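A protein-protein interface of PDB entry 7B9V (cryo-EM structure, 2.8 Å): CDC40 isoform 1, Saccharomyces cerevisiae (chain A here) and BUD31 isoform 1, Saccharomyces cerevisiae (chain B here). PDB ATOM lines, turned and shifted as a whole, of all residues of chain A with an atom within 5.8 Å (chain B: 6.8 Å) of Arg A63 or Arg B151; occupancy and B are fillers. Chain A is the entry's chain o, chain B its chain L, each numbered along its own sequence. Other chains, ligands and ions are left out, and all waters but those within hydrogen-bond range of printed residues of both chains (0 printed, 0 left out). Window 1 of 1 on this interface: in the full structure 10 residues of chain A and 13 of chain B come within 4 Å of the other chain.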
ATOM      1  N   ARG A  59      -7.963   0.120  16.392  1.00  0.00           N
ATOM      2  CA  ARG A  59      -8.614   1.330  16.900  1.00  0.00           C
ATOM      3  C   ARG A  59      -8.563   2.455  15.880  1.00  0.00           C
ATOM      4  O   ARG A  59      -9.493   3.269  15.812  1.00  0.00           O
ATOM      5  CB  ARG A  59      -7.999   1.778  18.227  1.00  0.00           C
ATOM      6  CG  ARG A  59      -8.221   0.819  19.386  1.00  0.00           C
ATOM      7  CD  ARG A  59      -9.165   1.326  20.422  1.00  0.00           C
ATOM      8  NE  ARG A  59      -8.580   2.492  21.066  1.00  0.00           N
ATOM      9  CZ  ARG A  59      -9.265   3.369  21.781  1.00  0.00           C
ATOM     10  NH1 ARG A  59     -10.567   3.240  21.966  1.00  0.00           N
ATOM     11  NH2 ARG A  59      -8.624   4.396  22.333  1.00  0.00           N
ATOM     12  N   ARG A  60      -7.422   2.590  15.176  1.00  0.00           N
ATOM     13  CA  ARG A  60      -7.304   3.574  14.100  1.00  0.00           C
ATOM     14  C   ARG A  60      -8.358   3.360  13.025  1.00  0.00           C
ATOM     15  O   ARG A  60      -8.914   4.328  12.492  1.00  0.00           O
ATOM     16  CB  ARG A  60      -5.906   3.495  13.488  1.00  0.00           C
ATOM     17  CG  ARG A  60      -4.827   4.111  14.340  1.00  0.00           C
ATOM     18  CD  ARG A  60      -3.588   4.451  13.511  1.00  0.00           C
ATOM     19  NE  ARG A  60      -2.885   3.278  12.998  1.00  0.00           N
ATOM     20  CZ  ARG A  60      -2.094   2.494  13.720  1.00  0.00           C
ATOM     21  NH1 ARG A  60      -1.886   2.709  15.009  1.00  0.00           N
ATOM     22  NH2 ARG A  60      -1.503   1.457  13.136  1.00  0.00           N
ATOM     23  N   LYS A  61      -8.614   2.091  12.672  1.00  0.00           N
ATOM     24  CA  LYS A  61      -9.550   1.772  11.601  1.00  0.00           C
ATOM     25  C   LYS A  61     -10.994   2.113  11.958  1.00  0.00           C
ATOM     26  O   LYS A  61     -11.827   2.238  11.057  1.00  0.00           O
ATOM     27  CB  LYS A  61      -9.434   0.295  11.221  1.00  0.00           C
ATOM     28  CG  LYS A  61      -8.817   0.041   9.843  1.00  0.00           C
ATOM     29  CD  LYS A  61      -7.402   0.584   9.710  1.00  0.00           C
ATOM     30  CE  LYS A  61      -6.828   0.272   8.332  1.00  0.00           C
ATOM     31  NZ  LYS A  61      -5.544   0.981   8.064  1.00  0.00           N
ATOM     32  N   THR A  62     -11.305   2.271  13.251  1.00  0.00           N
ATOM     33  CA  THR A  62     -12.656   2.614  13.675  1.00  0.00           C
ATOM     34  C   THR A  62     -12.997   4.084  13.504  1.00  0.00           C
ATOM     35  O   THR A  62     -14.179   4.429  13.614  1.00  0.00           O
ATOM     36  CB  THR A  62     -12.874   2.224  15.141  1.00  0.00           C
ATOM     37  OG1 THR A  62     -11.940   2.921  15.977  1.00  0.00           O
ATOM     38  CG2 THR A  62     -12.697   0.726  15.326  1.00  0.00           C
ATOM     39  N   ARG A  63     -12.004   4.946  13.284  1.00  0.00           N
ATOM     40  CA  ARG A  63     -12.253   6.377  13.168  1.00  0.00           C
ATOM     41  C   ARG A  63     -13.032   6.690  11.896  1.00  0.00           C
ATOM     42  O   ARG A  63     -12.717   6.183  10.816  1.00  0.00           O
ATOM     43  CB  ARG A  63     -10.938   7.154  13.184  1.00  0.00           C
ATOM     44  CG  ARG A  63     -10.208   7.111  14.517  1.00  0.00           C
ATOM     45  CD  ARG A  63      -8.977   7.997  14.504  1.00  0.00           C
ATOM     46  NE  ARG A  63      -9.327   9.411  14.579  1.00  0.00           N
ATOM     47  CZ  ARG A  63      -8.448  10.392  14.724  1.00  0.00           C
ATOM     48  NH1 ARG A  63      -7.150  10.148  14.818  1.00  0.00           N
ATOM     49  NH2 ARG A  63      -8.880  11.648  14.780  1.00  0.00           N
ATOM     50  N   LYS A  64     -14.048   7.544  12.022  1.00  0.00           N
ATOM     51  CA  LYS A  64     -14.848   7.955  10.868  1.00  0.00           C
ATOM     52  C   LYS A  64     -14.113   9.064  10.113  1.00  0.00           C
ATOM     53  O   LYS A  64     -14.461  10.244  10.170  1.00  0.00           O
ATOM     54  CB  LYS A  64     -16.235   8.402  11.309  1.00  0.00           C
ATOM     55  CG  LYS A  64     -17.073   7.322  11.980  1.00  0.00           C
ATOM     56  CD  LYS A  64     -18.550   7.704  12.001  1.00  0.00           C
ATOM     57  CE  LYS A  64     -18.817   8.911  12.889  1.00  0.00           C
ATOM     58  NZ  LYS A  64     -20.236   9.359  12.793  1.00  0.00           N
ATOM     59  N   GLY A  65     -13.078   8.666   9.398  1.00  0.00           N
ATOM     60  CA  GLY A  65     -12.297   9.589   8.601  1.00  0.00           C
ATOM     61  C   GLY A  65     -10.872   9.098   8.443  1.00  0.00           C
ATOM     62  O   GLY A  65     -10.318   8.402   9.289  1.00  0.00           O
ATOM     63  N   ASP A  66     -10.262   9.482   7.321  1.00  0.00           N
ATOM     64  CA  ASP A  66      -8.932   9.033   6.929  1.00  0.00           C
ATOM     65  C   ASP A  66      -7.837  10.047   7.259  1.00  0.00           C
ATOM     66  O   ASP A  66      -6.832  10.134   6.546  1.00  0.00           O
ATOM     67  CB  ASP A  66      -8.932   8.696   5.435  1.00  0.00           C
ATOM     68  CG  ASP A  66      -9.271   9.901   4.537  1.00  0.00           C
ATOM     69  OD1 ASP A  66      -9.706  10.971   5.024  1.00  0.00           O
ATOM     70  OD2 ASP A  66      -9.078   9.774   3.310  1.00  0.00           O
ATOM     71  N   GLY A  67      -8.006  10.802   8.335  1.00  0.00           N
ATOM     72  CA  GLY A  67      -7.032  11.786   8.735  1.00  0.00           C
ATOM     73  C   GLY A  67      -7.203  12.167  10.187  1.00  0.00           C
ATOM     74  O   GLY A  67      -7.915  11.495  10.939  1.00  0.00           O
ATOM     75  N   PRO A  68      -6.477  13.204  10.625  1.00  0.00           N
ATOM     76  CA  PRO A  68      -6.614  13.693  12.013  1.00  0.00           C
ATOM     77  C   PRO A  68      -8.015  14.180  12.378  1.00  0.00           C
ATOM     78  O   PRO A  68      -8.372  14.172  13.562  1.00  0.00           O
ATOM     79  CB  PRO A  68      -5.598  14.841  12.083  1.00  0.00           C
ATOM     80  CG  PRO A  68      -4.623  14.561  10.997  1.00  0.00           C
ATOM     81  CD  PRO A  68      -5.384  13.884   9.904  1.00  0.00           C
ATOM     82  N   TRP A  69      -8.814  14.598  11.400  1.00  0.00           N
ATOM     83  CA  TRP A  69     -10.167  15.087  11.615  1.00  0.00           C
ATOM     84  C   TRP A  69     -11.210  13.977  11.588  1.00  0.00           C
ATOM     85  O   TRP A  69     -12.409  14.271  11.611  1.00  0.00           O
ATOM     86  CB  TRP A  69     -10.503  16.160  10.576  1.00  0.00           C
ATOM     87  CG  TRP A  69      -9.759  17.429  10.829  1.00  0.00           C
ATOM     88  CD1 TRP A  69     -10.227  18.531  11.478  1.00  0.00           C
ATOM     89  CD2 TRP A  69      -8.409  17.729  10.448  1.00  0.00           C
ATOM     90  NE1 TRP A  69      -9.254  19.497  11.533  1.00  0.00           N
ATOM     91  CE2 TRP A  69      -8.130  19.031  10.905  1.00  0.00           C
ATOM     92  CE3 TRP A  69      -7.413  17.028   9.761  1.00  0.00           C
ATOM     93  CZ2 TRP A  69      -6.897  19.643  10.704  1.00  0.00           C
ATOM     94  CZ3 TRP A  69      -6.189  17.636   9.564  1.00  0.00           C
ATOM     95  CH2 TRP A  69      -5.942  18.932  10.033  1.00  0.00           C
ATOM     96  N   GLY A  70     -10.783  12.718  11.520  1.00  0.00           N
ATOM     97  CA  GLY A  70     -11.724  11.612  11.614  1.00  0.00           C
ATOM     98  C   GLY A  70     -12.273  11.463  13.024  1.00  0.00           C
ATOM     99  O   GLY A  70     -11.560  11.633  14.014  1.00  0.00           O
ATOM    100  N   SER A  71     -13.560  11.134  13.112  1.00  0.00           N
ATOM    101  CA  SER A  71     -14.260  11.176  14.386  1.00  0.00           C
ATOM    102  C   SER A  71     -14.320   9.824  15.082  1.00  0.00           C
ATOM    103  O   SER A  71     -14.341   8.766  14.447  1.00  0.00           O
ATOM    104  CB  SER A  71     -15.673  11.731  14.197  1.00  0.00           C
ATOM    105  OG  SER A  71     -16.358  11.796  15.434  1.00  0.00           O
ATOM    106  N   TRP A  72     -14.350   9.884  16.411  1.00  0.00           N
ATOM    107  CA  TRP A  72     -14.572   8.723  17.261  1.00  0.00           C
ATOM    108  C   TRP A  72     -16.018   8.570  17.710  1.00  0.00           C
ATOM    109  O   TRP A  72     -16.315   7.656  18.483  1.00  0.00           O
ATOM    110  CB  TRP A  72     -13.698   8.785  18.520  1.00  0.00           C
ATOM    111  CG  TRP A  72     -12.259   9.146  18.319  1.00  0.00           C
ATOM    112  CD1 TRP A  72     -11.740  10.398  18.136  1.00  0.00           C
ATOM    113  CD2 TRP A  72     -11.144   8.247  18.312  1.00  0.00           C
ATOM    114  NE1 TRP A  72     -10.377  10.331  18.004  1.00  0.00           N
ATOM    115  CE2 TRP A  72      -9.985   9.022  18.108  1.00  0.00           C
ATOM    116  CE3 TRP A  72     -11.012   6.861  18.451  1.00  0.00           C
ATOM    117  CZ2 TRP A  72      -8.712   8.461  18.046  1.00  0.00           C
ATOM    118  CZ3 TRP A  72      -9.746   6.304  18.384  1.00  0.00           C
ATOM    119  CH2 TRP A  72      -8.614   7.102  18.179  1.00  0.00           C
ATOM    120  N   SEP A  73     -16.892   9.474  17.261  1.00  0.00           N
ATOM    121  CA  SEP A  73     -18.266   9.570  17.771  1.00  0.00           C
ATOM    122  CB  SEP A  73     -18.948  10.844  17.259  1.00  0.00           C
ATOM    123  OG  SEP A  73     -18.330  12.001  17.806  1.00  0.00           O
ATOM    124  C   SEP A  73     -19.113   8.346  17.431  1.00  0.00           C
ATOM    125  O   SEP A  73     -18.789   7.583  16.521  1.00  0.00           O
ATOM    126  P   SEP A  73     -18.910  13.335  17.118  1.00  0.00           P
ATOM    127  O1P SEP A  73     -20.515  13.341  17.229  1.00  0.00           O
ATOM    128  O2P SEP A  73     -18.478  13.370  15.567  1.00  0.00           O
ATOM    129  O3P SEP A  73     -18.323  14.628  17.874  1.00  0.00           O
ATOM    130  N   CYS B 122      -5.081  17.622  21.666  1.00  0.00           N
ATOM    131  CA  CYS B 122      -5.249  16.680  20.566  1.00  0.00           C
ATOM    132  C   CYS B 122      -3.999  15.834  20.312  1.00  0.00           C
ATOM    133  O   CYS B 122      -4.099  14.814  19.620  1.00  0.00           O
ATOM    134  CB  CYS B 122      -5.661  17.449  19.299  1.00  0.00           C
ATOM    135  SG  CYS B 122      -4.318  18.307  18.427  1.00  0.00           S
ATOM    136  N   VAL B 124      -2.432  14.269  22.766  1.00  0.00           N
ATOM    137  CA  VAL B 124      -2.455  13.146  23.712  1.00  0.00           C
ATOM    138  C   VAL B 124      -2.991  11.921  22.988  1.00  0.00           C
ATOM    139  O   VAL B 124      -3.905  12.073  22.153  1.00  0.00           O
ATOM    140  CB  VAL B 124      -3.310  13.496  24.937  1.00  0.00           C
ATOM    141  CG1 VAL B 124      -3.288  12.385  25.990  1.00  0.00           C
ATOM    142  CG2 VAL B 124      -2.822  14.781  25.550  1.00  0.00           C
ATOM    143  N   ARG B 126      -5.357   8.866  22.369  1.00  0.00           N
ATOM    144  CA  ARG B 126      -6.756   8.751  22.781  1.00  0.00           C
ATOM    145  C   ARG B 126      -6.942   7.747  23.917  1.00  0.00           C
ATOM    146  O   ARG B 126      -7.848   7.917  24.747  1.00  0.00           O
ATOM    147  CB  ARG B 126      -7.619   8.382  21.573  1.00  0.00           C
ATOM    148  CG  ARG B 126      -9.126   8.481  21.798  1.00  0.00           C
ATOM    149  CD  ARG B 126      -9.599   9.920  21.901  1.00  0.00           C
ATOM    150  NE  ARG B 126     -11.044   9.991  22.074  1.00  0.00           N
ATOM    151  CZ  ARG B 126     -11.751  11.113  22.054  1.00  0.00           C
ATOM    152  NH1 ARG B 126     -11.177  12.289  21.856  1.00  0.00           N
ATOM    153  NH2 ARG B 126     -13.066  11.054  22.240  1.00  0.00           N
ATOM    154  N   LEU B 129      -6.379   9.509  27.334  1.00  0.00           N
ATOM    155  CA  LEU B 129      -7.543  10.288  27.748  1.00  0.00           C
ATOM    156  C   LEU B 129      -8.684   9.383  28.179  1.00  0.00           C
ATOM    157  O   LEU B 129      -9.418   9.710  29.122  1.00  0.00           O
ATOM    158  CB  LEU B 129      -7.999  11.206  26.613  1.00  0.00           C
ATOM    159  CG  LEU B 129      -7.064  12.300  26.102  1.00  0.00           C
ATOM    160  CD1 LEU B 129      -7.670  12.991  24.893  1.00  0.00           C
ATOM    161  CD2 LEU B 129      -6.770  13.309  27.202  1.00  0.00           C
ATOM    162  N   PHE B 142     -13.238  15.685  25.602  1.00  0.00           N
ATOM    163  CA  PHE B 142     -12.583  16.332  24.470  1.00  0.00           C
ATOM    164  C   PHE B 142     -13.129  15.790  23.153  1.00  0.00           C
ATOM    165  O   PHE B 142     -13.003  14.595  22.863  1.00  0.00           O
ATOM    166  CB  PHE B 142     -11.071  16.140  24.527  1.00  0.00           C
ATOM    167  CG  PHE B 142     -10.378  16.528  23.256  1.00  0.00           C
ATOM    168  CD1 PHE B 142     -10.421  17.840  22.806  1.00  0.00           C
ATOM    169  CD2 PHE B 142      -9.699  15.583  22.499  1.00  0.00           C
ATOM    170  CE1 PHE B 142      -9.800  18.197  21.632  1.00  0.00           C
ATOM    171  CE2 PHE B 142      -9.071  15.941  21.316  1.00  0.00           C
ATOM    172  CZ  PHE B 142      -9.126  17.252  20.884  1.00  0.00           C
ATOM    173  N   HIS B 143     -13.736  16.674  22.360  1.00  0.00           N
ATOM    174  CA  HIS B 143     -14.187  16.353  21.008  1.00  0.00           C
ATOM    175  C   HIS B 143     -13.276  16.946  19.934  1.00  0.00           C
ATOM    176  O   HIS B 143     -12.691  16.207  19.137  1.00  0.00           O
ATOM    177  CB  HIS B 143     -15.630  16.827  20.826  1.00  0.00           C
ATOM    178  CG  HIS B 143     -16.544  16.374  21.922  1.00  0.00           C
ATOM    179  ND1 HIS B 143     -17.057  15.097  21.987  1.00  0.00           N
ATOM    180  CD2 HIS B 143     -17.029  17.032  22.999  1.00  0.00           C
ATOM    181  CE1 HIS B 143     -17.819  14.988  23.062  1.00  0.00           C
ATOM    182  NE2 HIS B 143     -17.820  16.148  23.692  1.00  0.00           N
ATOM    183  N   GLN B 144     -13.129  18.274  19.914  1.00  0.00           N
ATOM    184  CA  GLN B 144     -12.357  18.979  18.897  1.00  0.00           C
ATOM    185  C   GLN B 144     -11.615  20.135  19.538  1.00  0.00           C
ATOM    186  O   GLN B 144     -12.180  20.870  20.353  1.00  0.00           O
ATOM    187  CB  GLN B 144     -13.250  19.533  17.782  1.00  0.00           C
ATOM    188  CG  GLN B 144     -13.640  18.511  16.759  1.00  0.00           C
ATOM    189  CD  GLN B 144     -14.592  19.010  15.702  1.00  0.00           C
ATOM    190  OE1 GLN B 144     -15.761  19.279  15.972  1.00  0.00           O
ATOM    191  NE2 GLN B 144     -14.095  19.128  14.476  1.00  0.00           N
ATOM    192  N   CYS B 145     -10.350  20.303  19.154  1.00  0.00           N
ATOM    193  CA  CYS B 145      -9.534  21.357  19.733  1.00  0.00           C
ATOM    194  C   CYS B 145      -9.765  22.677  19.011  1.00  0.00           C
ATOM    195  O   CYS B 145     -10.128  22.700  17.833  1.00  0.00           O
ATOM    196  CB  CYS B 145      -8.048  20.980  19.702  1.00  0.00           C
ATOM    197  SG  CYS B 145      -7.214  21.004  18.090  1.00  0.00           S
ATOM    198  N   CYS B 148      -7.617  24.133  15.386  1.00  0.00           N
ATOM    199  CA  CYS B 148      -7.860  23.639  14.041  1.00  0.00           C
ATOM    200  C   CYS B 148      -8.972  22.603  13.925  1.00  0.00           C
ATOM    201  O   CYS B 148      -9.181  22.088  12.822  1.00  0.00           O
ATOM    202  CB  CYS B 148      -6.563  23.082  13.457  1.00  0.00           C
ATOM    203  SG  CYS B 148      -6.014  21.635  14.303  1.00  0.00           S
ATOM    204  N   GLY B 149      -9.685  22.274  15.000  1.00  0.00           N
ATOM    205  CA  GLY B 149     -10.694  21.238  14.913  1.00  0.00           C
ATOM    206  C   GLY B 149     -10.216  19.811  14.866  1.00  0.00           C
ATOM    207  O   GLY B 149     -11.025  18.925  14.561  1.00  0.00           O
ATOM    208  N   CYS B 150      -8.928  19.572  15.095  1.00  0.00           N
ATOM    209  CA  CYS B 150      -8.389  18.219  15.103  1.00  0.00           C
ATOM    210  C   CYS B 150      -8.972  17.421  16.264  1.00  0.00           C
ATOM    211  O   CYS B 150      -9.148  17.936  17.371  1.00  0.00           O
ATOM    212  CB  CYS B 150      -6.863  18.250  15.194  1.00  0.00           C
ATOM    213  SG  CYS B 150      -6.062  16.688  15.601  1.00  0.00           S
ATOM    214  N   ARG B 151      -9.282  16.156  15.997  1.00  0.00           N
ATOM    215  CA  ARG B 151      -9.894  15.267  16.973  1.00  0.00           C
ATOM    216  C   ARG B 151      -8.900  14.296  17.575  1.00  0.00           C
ATOM    217  O   ARG B 151      -9.298  13.404  18.329  1.00  0.00           O
ATOM    218  CB  ARG B 151     -11.030  14.490  16.314  1.00  0.00           C
ATOM    219  CG  ARG B 151     -12.166  15.355  15.851  1.00  0.00           C
ATOM    220  CD  ARG B 151     -13.219  14.548  15.169  1.00  0.00           C
ATOM    221  NE  ARG B 151     -14.406  15.266  14.720  1.00  0.00           N
ATOM    222  CZ  ARG B 151     -15.525  15.371  15.425  1.00  0.00           C
ATOM    223  NH1 ARG B 151     -15.636  14.830  16.626  1.00  0.00           N
ATOM    224  NH2 ARG B 151     -16.566  16.007  14.898  1.00  0.00           N
ATOM    225  N   GLY B 152      -7.624  14.439  17.245  1.00  0.00           N
ATOM    226  CA  GLY B 152      -6.590  13.584  17.784  1.00  0.00           C
ATOM    227  C   GLY B 152      -5.564  13.240  16.731  1.00  0.00           C
ATOM    228  O   GLY B 152      -5.899  12.688  15.679  1.00  0.00           O
ATOM    229  N   CYS B 153      -4.305  13.567  16.994  1.00  0.00           N
ATOM    230  CA  CYS B 153      -3.246  13.369  16.014  1.00  0.00           C
ATOM    231  C   CYS B 153      -1.969  12.863  16.670  1.00  0.00           C
ATOM    232  O   CYS B 153      -0.858  13.192  16.244  1.00  0.00           O
ATOM    233  CB  CYS B 153      -3.013  14.641  15.205  1.00  0.00           C
ATOM    234  SG  CYS B 153      -2.437  16.024  16.183  1.00  0.00           S
ATOM    235  N   ALA B 154      -2.106  12.029  17.696  1.00  0.00           N
ATOM    236  CA  ALA B 154      -0.969  11.231  18.119  1.00  0.00           C
ATOM    237  C   ALA B 154      -0.708  10.176  17.058  1.00  0.00           C
ATOM    238  O   ALA B 154      -1.634   9.721  16.377  1.00  0.00           O
ATOM    239  CB  ALA B 154      -1.234  10.562  19.465  1.00  0.00           C
ATOM    240  N   ASP B 157      -2.599   7.074  16.670  1.00  0.00           N
ATOM    241  CA  ASP B 157      -4.011   7.244  16.339  1.00  0.00           C
ATOM    242  C   ASP B 157      -4.221   7.677  14.887  1.00  0.00           C
ATOM    243  O   ASP B 157      -5.333   8.025  14.485  1.00  0.00           O
ATOM    244  CB  ASP B 157      -4.647   8.269  17.278  1.00  0.00           C
ATOM    245  CG  ASP B 157      -4.443   7.932  18.746  1.00  0.00           C
ATOM    246  OD1 ASP B 157      -4.004   6.806  19.063  1.00  0.00           O
ATOM    247  OD2 ASP B 157      -4.695   8.813  19.591  1.00  0.00           O
ATOM    248  OXT ASP B 157      -3.300   7.669  14.070  1.00  0.00           O
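The guanidinium group (NH1) of Arg A63 lies within hydrogen-bond range of the backbone carbonyl oxygen (O) of Gly B152 (3.0 Å). The guanidinium group of Arg B151 sits at hydrogen-bond distance from the side-chain hydroxyl of Ser A71 (3.3 Å). The chain-end carboxylate of Asp B157 is in salt-bridge range of the guanidinium group of Arg A63 (2.8 Å). N of Arg B151 sits at hydrogen-bond distance from O of Pro A68, at 3.3 Å. The backbone carbonyl oxygen (O) of Arg B151 lies within hydrogen-bond range of the indole nitrogen (NE1) of Trp A72, at 3.3 Å. NH1 of Arg B151 sits close to O3P of SEP A73. The indole nitrogen (NE1) of Trp A69 lies within hydrogen-bond range of the backbone carbonyl oxygen (O) of Cys B148, 2.9 Å away.
The side-chain sulfur (SG) of Cys B150 lies close to the backbone NH (N) of Gly B152 (3.2 Å). OD2 of Asp B157 sits at hydrogen-bond distance from N of Arg B126, 2.9 Å away. SG of Cys B148 sits close to N of Cys B150 (3.7 Å). NE2 of Gln B144 sits at hydrogen-bond distance from O of Gly B149 (3.1 Å). The side-chain hydroxyl (OG) of Ser A71 lies within hydrogen-bond range of O2P of SEP A73, at 2.6 Å. The backbone NH of Lys A64 sits at hydrogen-bond distance from the backbone carbonyl oxygen of Ser A71 (2.7 Å).
Arg A60 touches Asp B157 (CD to OXT, 3.3 Å). NH2 of Arg A63 touches C of Arg B151, at 3.9 Å. Pro A68 touches Cys B150. O of Pro A68 touches O of Gly B152, 3.6 Å away. Trp A69 touches Gly B149. N of Cys B150 touches NE1 of Trp A69, 3.6 Å away. CD of Arg B151 touches O of Trp A69, at 3.7 Å. Gly A70 touches Arg B151. Trp A72 touches Arg B126 (CZ2 to CB, 3.7 Å).
Arg A63 touches just these residues of chain B: Arg B151, Gly B152 and Asp B157. Arg B151 touches just these residues of chain A: Arg A63 (3.9 Å), Pro A68 (3.3 Å), Trp A69 (3.7 Å), Gly A70 (3.5 Å), Ser A71 (3.3 Å), Trp A72 (3.3 Å) and SEP A73 (3.0 Å). Printed residues of chain A within 4 Å of Cys B150: Pro A68 (3.98 Å) and Trp A69 (3.6 Å). Of the printed residues of chain B, Gly A70 touches Arg B151. Printed residues of chain B within 4 Å of Trp A69: Cys B148 (2.9 Å), Gly B149 (3.2 Å), Cys B150 (3.6 Å) and Arg B151 (3.7 Å).
Printed residues of chain A that touch a printed residue of chain B: Arg A60, Arg A63, Pro A68, Trp A69, Gly A70, Ser A71, Trp A72 and SEP A73.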
